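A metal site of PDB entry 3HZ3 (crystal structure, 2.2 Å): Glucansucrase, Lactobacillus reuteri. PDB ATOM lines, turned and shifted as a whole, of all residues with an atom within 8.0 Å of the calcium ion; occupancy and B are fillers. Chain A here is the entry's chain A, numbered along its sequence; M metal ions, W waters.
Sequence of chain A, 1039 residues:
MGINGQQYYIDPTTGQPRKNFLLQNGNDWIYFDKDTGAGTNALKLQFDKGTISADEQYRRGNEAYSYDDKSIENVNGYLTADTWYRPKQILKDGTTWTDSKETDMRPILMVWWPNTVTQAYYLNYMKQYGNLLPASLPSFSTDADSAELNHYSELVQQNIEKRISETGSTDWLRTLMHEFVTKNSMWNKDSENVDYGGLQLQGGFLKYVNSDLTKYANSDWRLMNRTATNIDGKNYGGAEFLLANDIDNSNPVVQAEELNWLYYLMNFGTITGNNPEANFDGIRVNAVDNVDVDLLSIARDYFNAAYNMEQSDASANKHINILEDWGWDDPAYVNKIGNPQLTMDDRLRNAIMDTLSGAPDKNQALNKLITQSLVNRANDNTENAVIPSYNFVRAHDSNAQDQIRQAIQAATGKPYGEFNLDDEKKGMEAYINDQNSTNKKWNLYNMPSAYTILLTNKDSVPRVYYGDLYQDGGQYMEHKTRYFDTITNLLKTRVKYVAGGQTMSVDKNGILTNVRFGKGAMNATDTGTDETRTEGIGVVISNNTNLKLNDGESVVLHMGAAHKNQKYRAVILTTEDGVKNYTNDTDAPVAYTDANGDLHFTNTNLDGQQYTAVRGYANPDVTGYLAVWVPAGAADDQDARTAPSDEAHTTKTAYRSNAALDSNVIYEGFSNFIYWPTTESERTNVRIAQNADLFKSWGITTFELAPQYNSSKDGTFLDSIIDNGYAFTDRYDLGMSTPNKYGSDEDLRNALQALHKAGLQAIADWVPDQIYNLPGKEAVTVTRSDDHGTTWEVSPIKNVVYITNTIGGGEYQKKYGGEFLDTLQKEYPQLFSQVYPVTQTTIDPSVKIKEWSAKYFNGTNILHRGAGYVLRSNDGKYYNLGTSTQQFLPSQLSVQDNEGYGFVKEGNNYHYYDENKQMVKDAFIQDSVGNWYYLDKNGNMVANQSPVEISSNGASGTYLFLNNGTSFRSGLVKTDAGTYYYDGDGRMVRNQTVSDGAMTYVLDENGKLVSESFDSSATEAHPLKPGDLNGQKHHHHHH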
ATOM      1  N   LEU A 223       7.582  16.555  -5.692  1.00  0.00           N
ATOM      2  CA  LEU A 223       7.191  17.850  -6.267  1.00  0.00           C
ATOM      3  C   LEU A 223       6.895  17.627  -7.753  1.00  0.00           C
ATOM      4  O   LEU A 223       7.793  17.282  -8.521  1.00  0.00           O
ATOM      5  CB  LEU A 223       8.301  18.914  -6.036  1.00  0.00           C
ATOM      6  CG  LEU A 223       8.731  19.155  -4.572  1.00  0.00           C
ATOM      7  CD1 LEU A 223       9.731  20.298  -4.402  1.00  0.00           C
ATOM      8  CD2 LEU A 223       7.520  19.411  -3.656  1.00  0.00           C
ATOM      9  N   MET A 224       5.621  17.808  -8.145  1.00  0.00           N
ATOM     10  CA  MET A 224       5.120  17.389  -9.453  1.00  0.00           C
ATOM     11  C   MET A 224       4.880  18.507 -10.474  1.00  0.00           C
ATOM     12  O   MET A 224       4.432  19.588 -10.097  1.00  0.00           O
ATOM     13  CB  MET A 224       3.805  16.601  -9.274  1.00  0.00           C
ATOM     14  CG  MET A 224       4.002  15.235  -8.612  1.00  0.00           C
ATOM     15  SD  MET A 224       2.533  14.173  -8.568  1.00  0.00           S
ATOM     16  CE  MET A 224       1.601  14.871  -7.183  1.00  0.00           C
ATOM     17  N   ASN A 225       5.102  18.218 -11.763  1.00  0.00           N
ATOM     18  CA  ASN A 225       4.810  19.167 -12.841  1.00  0.00           C
ATOM     19  C   ASN A 225       5.672  20.440 -12.809  1.00  0.00           C
ATOM     20  O   ASN A 225       5.284  21.476 -13.342  1.00  0.00           O
ATOM     21  CB  ASN A 225       3.342  19.631 -12.835  1.00  0.00           C
ATOM     22  CG  ASN A 225       2.378  18.523 -12.528  1.00  0.00           C
ATOM     23  OD1 ASN A 225       2.433  17.463 -13.131  1.00  0.00           O
ATOM     24  ND2 ASN A 225       1.493  18.755 -11.559  1.00  0.00           N
ATOM     25  N   GLY A 238       3.996  21.339 -17.249  1.00  0.00           N
ATOM     26  CA  GLY A 238       3.818  20.163 -18.077  1.00  0.00           C
ATOM     27  C   GLY A 238       3.427  18.970 -17.215  1.00  0.00           C
ATOM     28  O   GLY A 238       3.537  19.023 -15.987  1.00  0.00           O
ATOM     29  N   ALA A 239       2.997  17.890 -17.854  1.00  0.00           N
ATOM     30  CA  ALA A 239       2.484  16.733 -17.116  1.00  0.00           C
ATOM     31  C   ALA A 239       3.622  15.873 -16.522  1.00  0.00           C
ATOM     32  O   ALA A 239       4.501  15.379 -17.248  1.00  0.00           O
ATOM     33  CB  ALA A 239       1.579  15.900 -18.002  1.00  0.00           C
ATOM     34  N   GLU A 240       3.604  15.719 -15.206  1.00  0.00           N
ATOM     35  CA  GLU A 240       4.623  14.895 -14.555  1.00  0.00           C
ATOM     36  C   GLU A 240       4.543  13.457 -15.004  1.00  0.00           C
ATOM     37  O   GLU A 240       5.574  12.791 -15.132  1.00  0.00           O
ATOM     38  CB  GLU A 240       4.434  14.956 -13.052  1.00  0.00           C
ATOM     39  CG  GLU A 240       5.552  14.273 -12.274  1.00  0.00           C
ATOM     40  CD  GLU A 240       6.927  14.918 -12.463  1.00  0.00           C
ATOM     41  OE1 GLU A 240       7.044  16.159 -12.219  1.00  0.00           O
ATOM     42  OE2 GLU A 240       7.884  14.166 -12.816  1.00  0.00           O
ATOM     43  N   PHE A 241       3.311  12.966 -15.223  1.00  0.00           N
ATOM     44  CA  PHE A 241       3.118  11.560 -15.511  1.00  0.00           C
ATOM     45  C   PHE A 241       3.084  11.278 -17.021  1.00  0.00           C
ATOM     46  O   PHE A 241       2.470  12.039 -17.762  1.00  0.00           O
ATOM     47  CB  PHE A 241       1.850  11.051 -14.819  1.00  0.00           C
ATOM     48  CG  PHE A 241       2.001  10.936 -13.302  1.00  0.00           C
ATOM     49  CD1 PHE A 241       2.698   9.868 -12.727  1.00  0.00           C
ATOM     50  CD2 PHE A 241       1.417  11.887 -12.447  1.00  0.00           C
ATOM     51  CE1 PHE A 241       2.832   9.765 -11.320  1.00  0.00           C
ATOM     52  CE2 PHE A 241       1.552  11.794 -11.067  1.00  0.00           C
ATOM     53  CZ  PHE A 241       2.259  10.728 -10.491  1.00  0.00           C
ATOM     54  N   LEU A 242       3.755  10.190 -17.444  1.00  0.00           N
ATOM     55  CA  LEU A 242       3.876   9.841 -18.875  1.00  0.00           C
ATOM     56  C   LEU A 242       3.749   8.329 -19.121  1.00  0.00           C
ATOM     57  O   LEU A 242       2.820   7.891 -19.789  1.00  0.00           O
ATOM     58  CB  LEU A 242       5.199  10.383 -19.491  1.00  0.00           C
ATOM     59  CG  LEU A 242       5.488  10.122 -20.991  1.00  0.00           C
ATOM     60  CD1 LEU A 242       4.420  10.707 -21.914  1.00  0.00           C
ATOM     61  CD2 LEU A 242       6.847  10.656 -21.425  1.00  0.00           C
ATOM     62  N   LEU A 243       4.677   7.543 -18.599  1.00  0.00           N
ATOM     63  CA  LEU A 243       4.732   6.107 -18.848  1.00  0.00           C
ATOM     64  C   LEU A 243       5.294   5.409 -17.620  1.00  0.00           C
ATOM     65  O   LEU A 243       6.205   5.944 -16.955  1.00  0.00           O
ATOM     66  CB  LEU A 243       5.655   5.793 -20.041  1.00  0.00           C
ATOM     67  CG  LEU A 243       5.144   6.193 -21.436  1.00  0.00           C
ATOM     68  CD1 LEU A 243       6.252   6.245 -22.405  1.00  0.00           C
ATOM     69  CD2 LEU A 243       3.975   5.260 -21.933  1.00  0.00           C
ATOM     70  N   ASN A 245       6.864   3.520 -14.471  1.00  0.00           N
ATOM     71  CA  ASN A 245       7.151   4.062 -13.134  1.00  0.00           C
ATOM     72  C   ASN A 245       7.810   5.446 -13.189  1.00  0.00           C
ATOM     73  O   ASN A 245       8.967   5.567 -13.526  1.00  0.00           O
ATOM     74  CB  ASN A 245       8.028   3.082 -12.355  1.00  0.00           C
ATOM     75  CG  ASN A 245       7.465   1.698 -12.390  1.00  0.00           C
ATOM     76  OD1 ASN A 245       6.515   1.401 -11.687  1.00  0.00           O
ATOM     77  ND2 ASN A 245       8.029   0.843 -13.227  1.00  0.00           N
ATOM     78  N   ASP A 246       7.065   6.475 -12.824  1.00  0.00           N
ATOM     79  CA  ASP A 246       7.580   7.828 -12.909  1.00  0.00           C
ATOM     80  C   ASP A 246       8.583   8.140 -11.806  1.00  0.00           C
ATOM     81  O   ASP A 246       8.255   8.082 -10.606  1.00  0.00           O
ATOM     82  CB  ASP A 246       6.436   8.855 -12.906  1.00  0.00           C
ATOM     83  CG  ASP A 246       6.897  10.232 -13.364  1.00  0.00           C
ATOM     84  OD1 ASP A 246       7.192  10.457 -14.558  1.00  0.00           O
ATOM     85  OD2 ASP A 246       6.960  11.149 -12.533  1.00  0.00           O
ATOM     86  N   ILE A 247       9.775   8.510 -12.215  1.00  0.00           N
ATOM     87  CA  ILE A 247      10.863   8.831 -11.275  1.00  0.00           C
ATOM     88  C   ILE A 247      10.640  10.176 -10.596  1.00  0.00           C
ATOM     89  O   ILE A 247      10.403  11.165 -11.264  1.00  0.00           O
ATOM     90  CB  ILE A 247      12.228   8.726 -11.966  1.00  0.00           C
ATOM     91  CG1 ILE A 247      12.576   7.259 -12.144  1.00  0.00           C
ATOM     92  CG2 ILE A 247      13.318   9.385 -11.136  1.00  0.00           C
ATOM     93  CD1 ILE A 247      13.841   7.009 -13.016  1.00  0.00           C
ATOM     94  N   ASP A 248      10.716  10.218  -9.269  1.00  0.00           N
ATOM     95  CA  ASP A 248      10.644  11.492  -8.544  1.00  0.00           C
ATOM     96  C   ASP A 248      11.979  12.255  -8.617  1.00  0.00           C
ATOM     97  O   ASP A 248      12.861  12.064  -7.783  1.00  0.00           O
ATOM     98  CB  ASP A 248      10.266  11.271  -7.068  1.00  0.00           C
ATOM     99  CG  ASP A 248      10.131  12.578  -6.306  1.00  0.00           C
ATOM    100  OD1 ASP A 248       9.983  13.630  -6.959  1.00  0.00           O
ATOM    101  OD2 ASP A 248      10.117  12.553  -5.048  1.00  0.00           O
ATOM    102  N   ASN A 249      12.100  13.129  -9.609  1.00  0.00           N
ATOM    103  CA  ASN A 249      13.319  13.903  -9.816  1.00  0.00           C
ATOM    104  C   ASN A 249      13.368  15.177  -9.006  1.00  0.00           C
ATOM    105  O   ASN A 249      14.285  15.992  -9.167  1.00  0.00           O
ATOM    106  CB  ASN A 249      13.526  14.186 -11.327  1.00  0.00           C
ATOM    107  CG  ASN A 249      13.945  12.943 -12.075  1.00  0.00           C
ATOM    108  OD1 ASN A 249      13.160  12.314 -12.779  1.00  0.00           O
ATOM    109  ND2 ASN A 249      15.195  12.558 -11.887  1.00  0.00           N
ATOM    110  N   ALA A 287      12.062  13.849 -22.800  1.00  0.00           N
ATOM    111  CA  ALA A 287      10.837  14.117 -22.017  1.00  0.00           C
ATOM    112  C   ALA A 287      11.009  15.231 -20.992  1.00  0.00           C
ATOM    113  O   ALA A 287      10.659  15.091 -19.817  1.00  0.00           O
ATOM    114  CB  ALA A 287      10.337  12.832 -21.340  1.00  0.00           C
ATOM    115  N   VAL A 288      11.528  16.359 -21.446  1.00  0.00           N
ATOM    116  CA  VAL A 288      11.824  17.508 -20.611  1.00  0.00           C
ATOM    117  C   VAL A 288      10.612  18.080 -19.897  1.00  0.00           C
ATOM    118  O   VAL A 288      10.690  18.441 -18.717  1.00  0.00           O
ATOM    119  CB  VAL A 288      12.459  18.648 -21.460  1.00  0.00           C
ATOM    120  CG1 VAL A 288      12.619  19.921 -20.635  1.00  0.00           C
ATOM    121  CG2 VAL A 288      13.783  18.183 -21.960  1.00  0.00           C
ATOM    122  N   ASP A 289       9.498  18.212 -20.612  1.00  0.00           N
ATOM    123  CA  ASP A 289       8.307  18.757 -20.004  1.00  0.00           C
ATOM    124  C   ASP A 289       7.587  17.768 -19.054  1.00  0.00           C
ATOM    125  O   ASP A 289       6.472  18.042 -18.608  1.00  0.00           O
ATOM    126  CB  ASP A 289       7.396  19.381 -21.067  1.00  0.00           C
ATOM    127  CG  ASP A 289       7.983  20.679 -21.651  1.00  0.00           C
ATOM    128  OD1 ASP A 289       8.918  21.264 -21.004  1.00  0.00           O
ATOM    129  OD2 ASP A 289       7.509  21.119 -22.718  1.00  0.00           O
ATOM    130  N   ASN A 290       8.262  16.666 -18.705  1.00  0.00           N
ATOM    131  CA  ASN A 290       7.682  15.646 -17.831  1.00  0.00           C
ATOM    132  C   ASN A 290       8.482  15.403 -16.576  1.00  0.00           C
ATOM    133  O   ASN A 290       8.204  14.460 -15.825  1.00  0.00           O
ATOM    134  CB  ASN A 290       7.510  14.348 -18.613  1.00  0.00           C
ATOM    135  CG  ASN A 290       6.677  14.538 -19.852  1.00  0.00           C
ATOM    136  OD1 ASN A 290       7.157  14.343 -20.989  1.00  0.00           O
ATOM    137  ND2 ASN A 290       5.400  14.937 -19.659  1.00  0.00           N
ATOM    138  N   VAL A 291       9.496  16.225 -16.357  1.00  0.00           N
ATOM    139  CA  VAL A 291      10.334  16.059 -15.185  1.00  0.00           C
ATOM    140  C   VAL A 291      10.631  17.424 -14.572  1.00  0.00           C
ATOM    141  O   VAL A 291      10.417  18.480 -15.198  1.00  0.00           O
ATOM    142  CB  VAL A 291      11.691  15.353 -15.522  1.00  0.00           C
ATOM    143  CG1 VAL A 291      11.444  13.962 -16.087  1.00  0.00           C
ATOM    144  CG2 VAL A 291      12.584  16.207 -16.493  1.00  0.00           C
ATOM    145  N   ASP A 292      11.154  17.365 -13.354  1.00  0.00           N
ATOM    146  CA  ASP A 292      11.550  18.561 -12.630  1.00  0.00           C
ATOM    147  C   ASP A 292      12.689  19.265 -13.397  1.00  0.00           C
ATOM    148  O   ASP A 292      13.774  18.742 -13.589  1.00  0.00           O
ATOM    149  CB  ASP A 292      11.914  18.178 -11.165  1.00  0.00           C
ATOM    150  CG  ASP A 292      12.605  19.299 -10.394  1.00  0.00           C
ATOM    151  OD1 ASP A 292      12.690  20.426 -10.903  1.00  0.00           O
ATOM    152  OD2 ASP A 292      13.036  19.068  -9.230  1.00  0.00           O
ATOM    153  N   PRO A 768      15.775  10.233 -17.827  1.00  0.00           N
ATOM    154  CA  PRO A 768      15.521  10.227 -16.354  1.00  0.00           C
ATOM    155  C   PRO A 768      14.031  10.288 -15.953  1.00  0.00           C
ATOM    156  O   PRO A 768      13.700  10.401 -14.744  1.00  0.00           O
ATOM    157  CB  PRO A 768      16.161  11.545 -15.921  1.00  0.00           C
ATOM    158  CG  PRO A 768      15.811  12.475 -17.140  1.00  0.00           C
ATOM    159  CD  PRO A 768      16.071  11.591 -18.327  1.00  0.00           C
ATOM    160  N   ASP A 769      13.137  10.282 -16.936  1.00  0.00           N
ATOM    161  CA  ASP A 769      11.687  10.287 -16.591  1.00  0.00           C
ATOM    162  C   ASP A 769      11.190   9.042 -15.853  1.00  0.00           C
ATOM    163  O   ASP A 769      10.393   9.173 -14.930  1.00  0.00           O
ATOM    164  CB  ASP A 769      10.773  10.489 -17.786  1.00  0.00           C
ATOM    165  CG  ASP A 769       9.328  10.781 -17.358  1.00  0.00           C
ATOM    166  OD1 ASP A 769       8.397  10.016 -17.731  1.00  0.00           O
ATOM    167  OD2 ASP A 769       9.141  11.773 -16.609  1.00  0.00           O
ATOM    168  N   GLN A 770      11.594   7.866 -16.298  1.00  0.00           N
ATOM    169  CA  GLN A 770      10.890   6.635 -15.919  1.00  0.00           C
ATOM    170  C   GLN A 770      11.727   5.372 -16.121  1.00  0.00           C
ATOM    171  O   GLN A 770      12.843   5.427 -16.651  1.00  0.00           O
ATOM    172  CB  GLN A 770       9.544   6.499 -16.666  1.00  0.00           C
ATOM    173  CG  GLN A 770       9.646   5.924 -18.099  1.00  0.00           C
ATOM    174  CD  GLN A 770      10.006   6.963 -19.179  1.00  0.00           C
ATOM    175  OE1 GLN A 770       9.423   8.048 -19.219  1.00  0.00           O
ATOM    176  NE2 GLN A 770      10.953   6.610 -20.067  1.00  0.00           N
ATOM    177  N   ASP A 787      -2.630  12.975 -15.547  1.00  0.00           N
ATOM    178  CA  ASP A 787      -1.205  13.075 -15.856  1.00  0.00           C
ATOM    179  C   ASP A 787      -0.429  14.175 -15.146  1.00  0.00           C
ATOM    180  O   ASP A 787       0.787  14.260 -15.272  1.00  0.00           O
ATOM    181  CB  ASP A 787      -0.989  13.169 -17.391  1.00  0.00           C
ATOM    182  CG  ASP A 787      -1.632  14.421 -18.015  1.00  0.00           C
ATOM    183  OD1 ASP A 787      -2.030  15.340 -17.271  1.00  0.00           O
ATOM    184  OD2 ASP A 787      -1.684  14.511 -19.262  1.00  0.00           O
ATOM    185  N   ASN A 858       7.089   8.951  -8.263  1.00  0.00           N
ATOM    186  CA  ASN A 858       5.964   9.876  -8.107  1.00  0.00           C
ATOM    187  C   ASN A 858       4.690   9.053  -8.240  1.00  0.00           C
ATOM    188  O   ASN A 858       3.636   9.438  -7.719  1.00  0.00           O
ATOM    189  CB  ASN A 858       6.016  10.964  -9.192  1.00  0.00           C
ATOM    190  CG  ASN A 858       7.017  12.107  -8.887  1.00  0.00           C
ATOM    191  OD1 ASN A 858       7.285  12.459  -7.727  1.00  0.00           O
ATOM    192  ND2 ASN A 858       7.550  12.700  -9.936  1.00  0.00           N
HETATM  193 CA    CA M   1       7.908  12.632 -14.637  1.00  0.00          CA
HETATM  194  O   HOH W   1       9.900  11.662 -13.905  1.00  0.00           O
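The backbone carbonyl oxygen of Ala 239 lies within hydrogen-bond range of the side-chain amide nitrogen of Asn 290 (2.6 Å).
The backbone carbonyl oxygen (O) of Asp 246 sits at hydrogen-bond distance from the backbone NH (N) of Asn 858, 2.8 Å away.
The side-chain amide nitrogen of Asn 858 sits close to the side-chain carboxylate of Glu 240 (3.2 Å).
The side-chain carboxylate (OE1) of Glu 240 is in hydrogen-bond range of the backbone NH (N) of Asn 225, 2.9 Å away.
The backbone NH of Glu 240 is in hydrogen-bond range of the backbone carbonyl oxygen of Asp 787 (3.2 Å).
N of Ile 247 lies within hydrogen-bond range of O of Asp 769, 2.9 Å away.
The side-chain carboxylate of Asp 769 sits close to the side-chain amide oxygen of Gln 770 (2.7 Å).
Four residues have an atom within 4 Å of the calcium ion: Glu 240, Asp 246, Asn 290 and Asp 769.
The calcium ion is bound by O of Asn 290 (2.2 Å).
OD1 of Asp 246 is bound to the calcium ion, at 2.3 Å.
Water W1 binds the calcium ion (2.3 Å).
The calcium ion is bound by the side-chain carboxylate (OE2) of Glu 240, at 2.4 Å.
O of Glu 240 is bound to the calcium ion (2.4 Å).
The side-chain carboxylate (OD2) of Asp 769 is bound to the calcium ion.
OD2 of Asp 246 binds the calcium ion, at 2.7 Å.
The calcium ion has seven donor atoms within binding distance.
Water W1 bridges the backbone carbonyl oxygen (O) of Ile 247 and the backbone carbonyl oxygen (O) of Asp 769.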
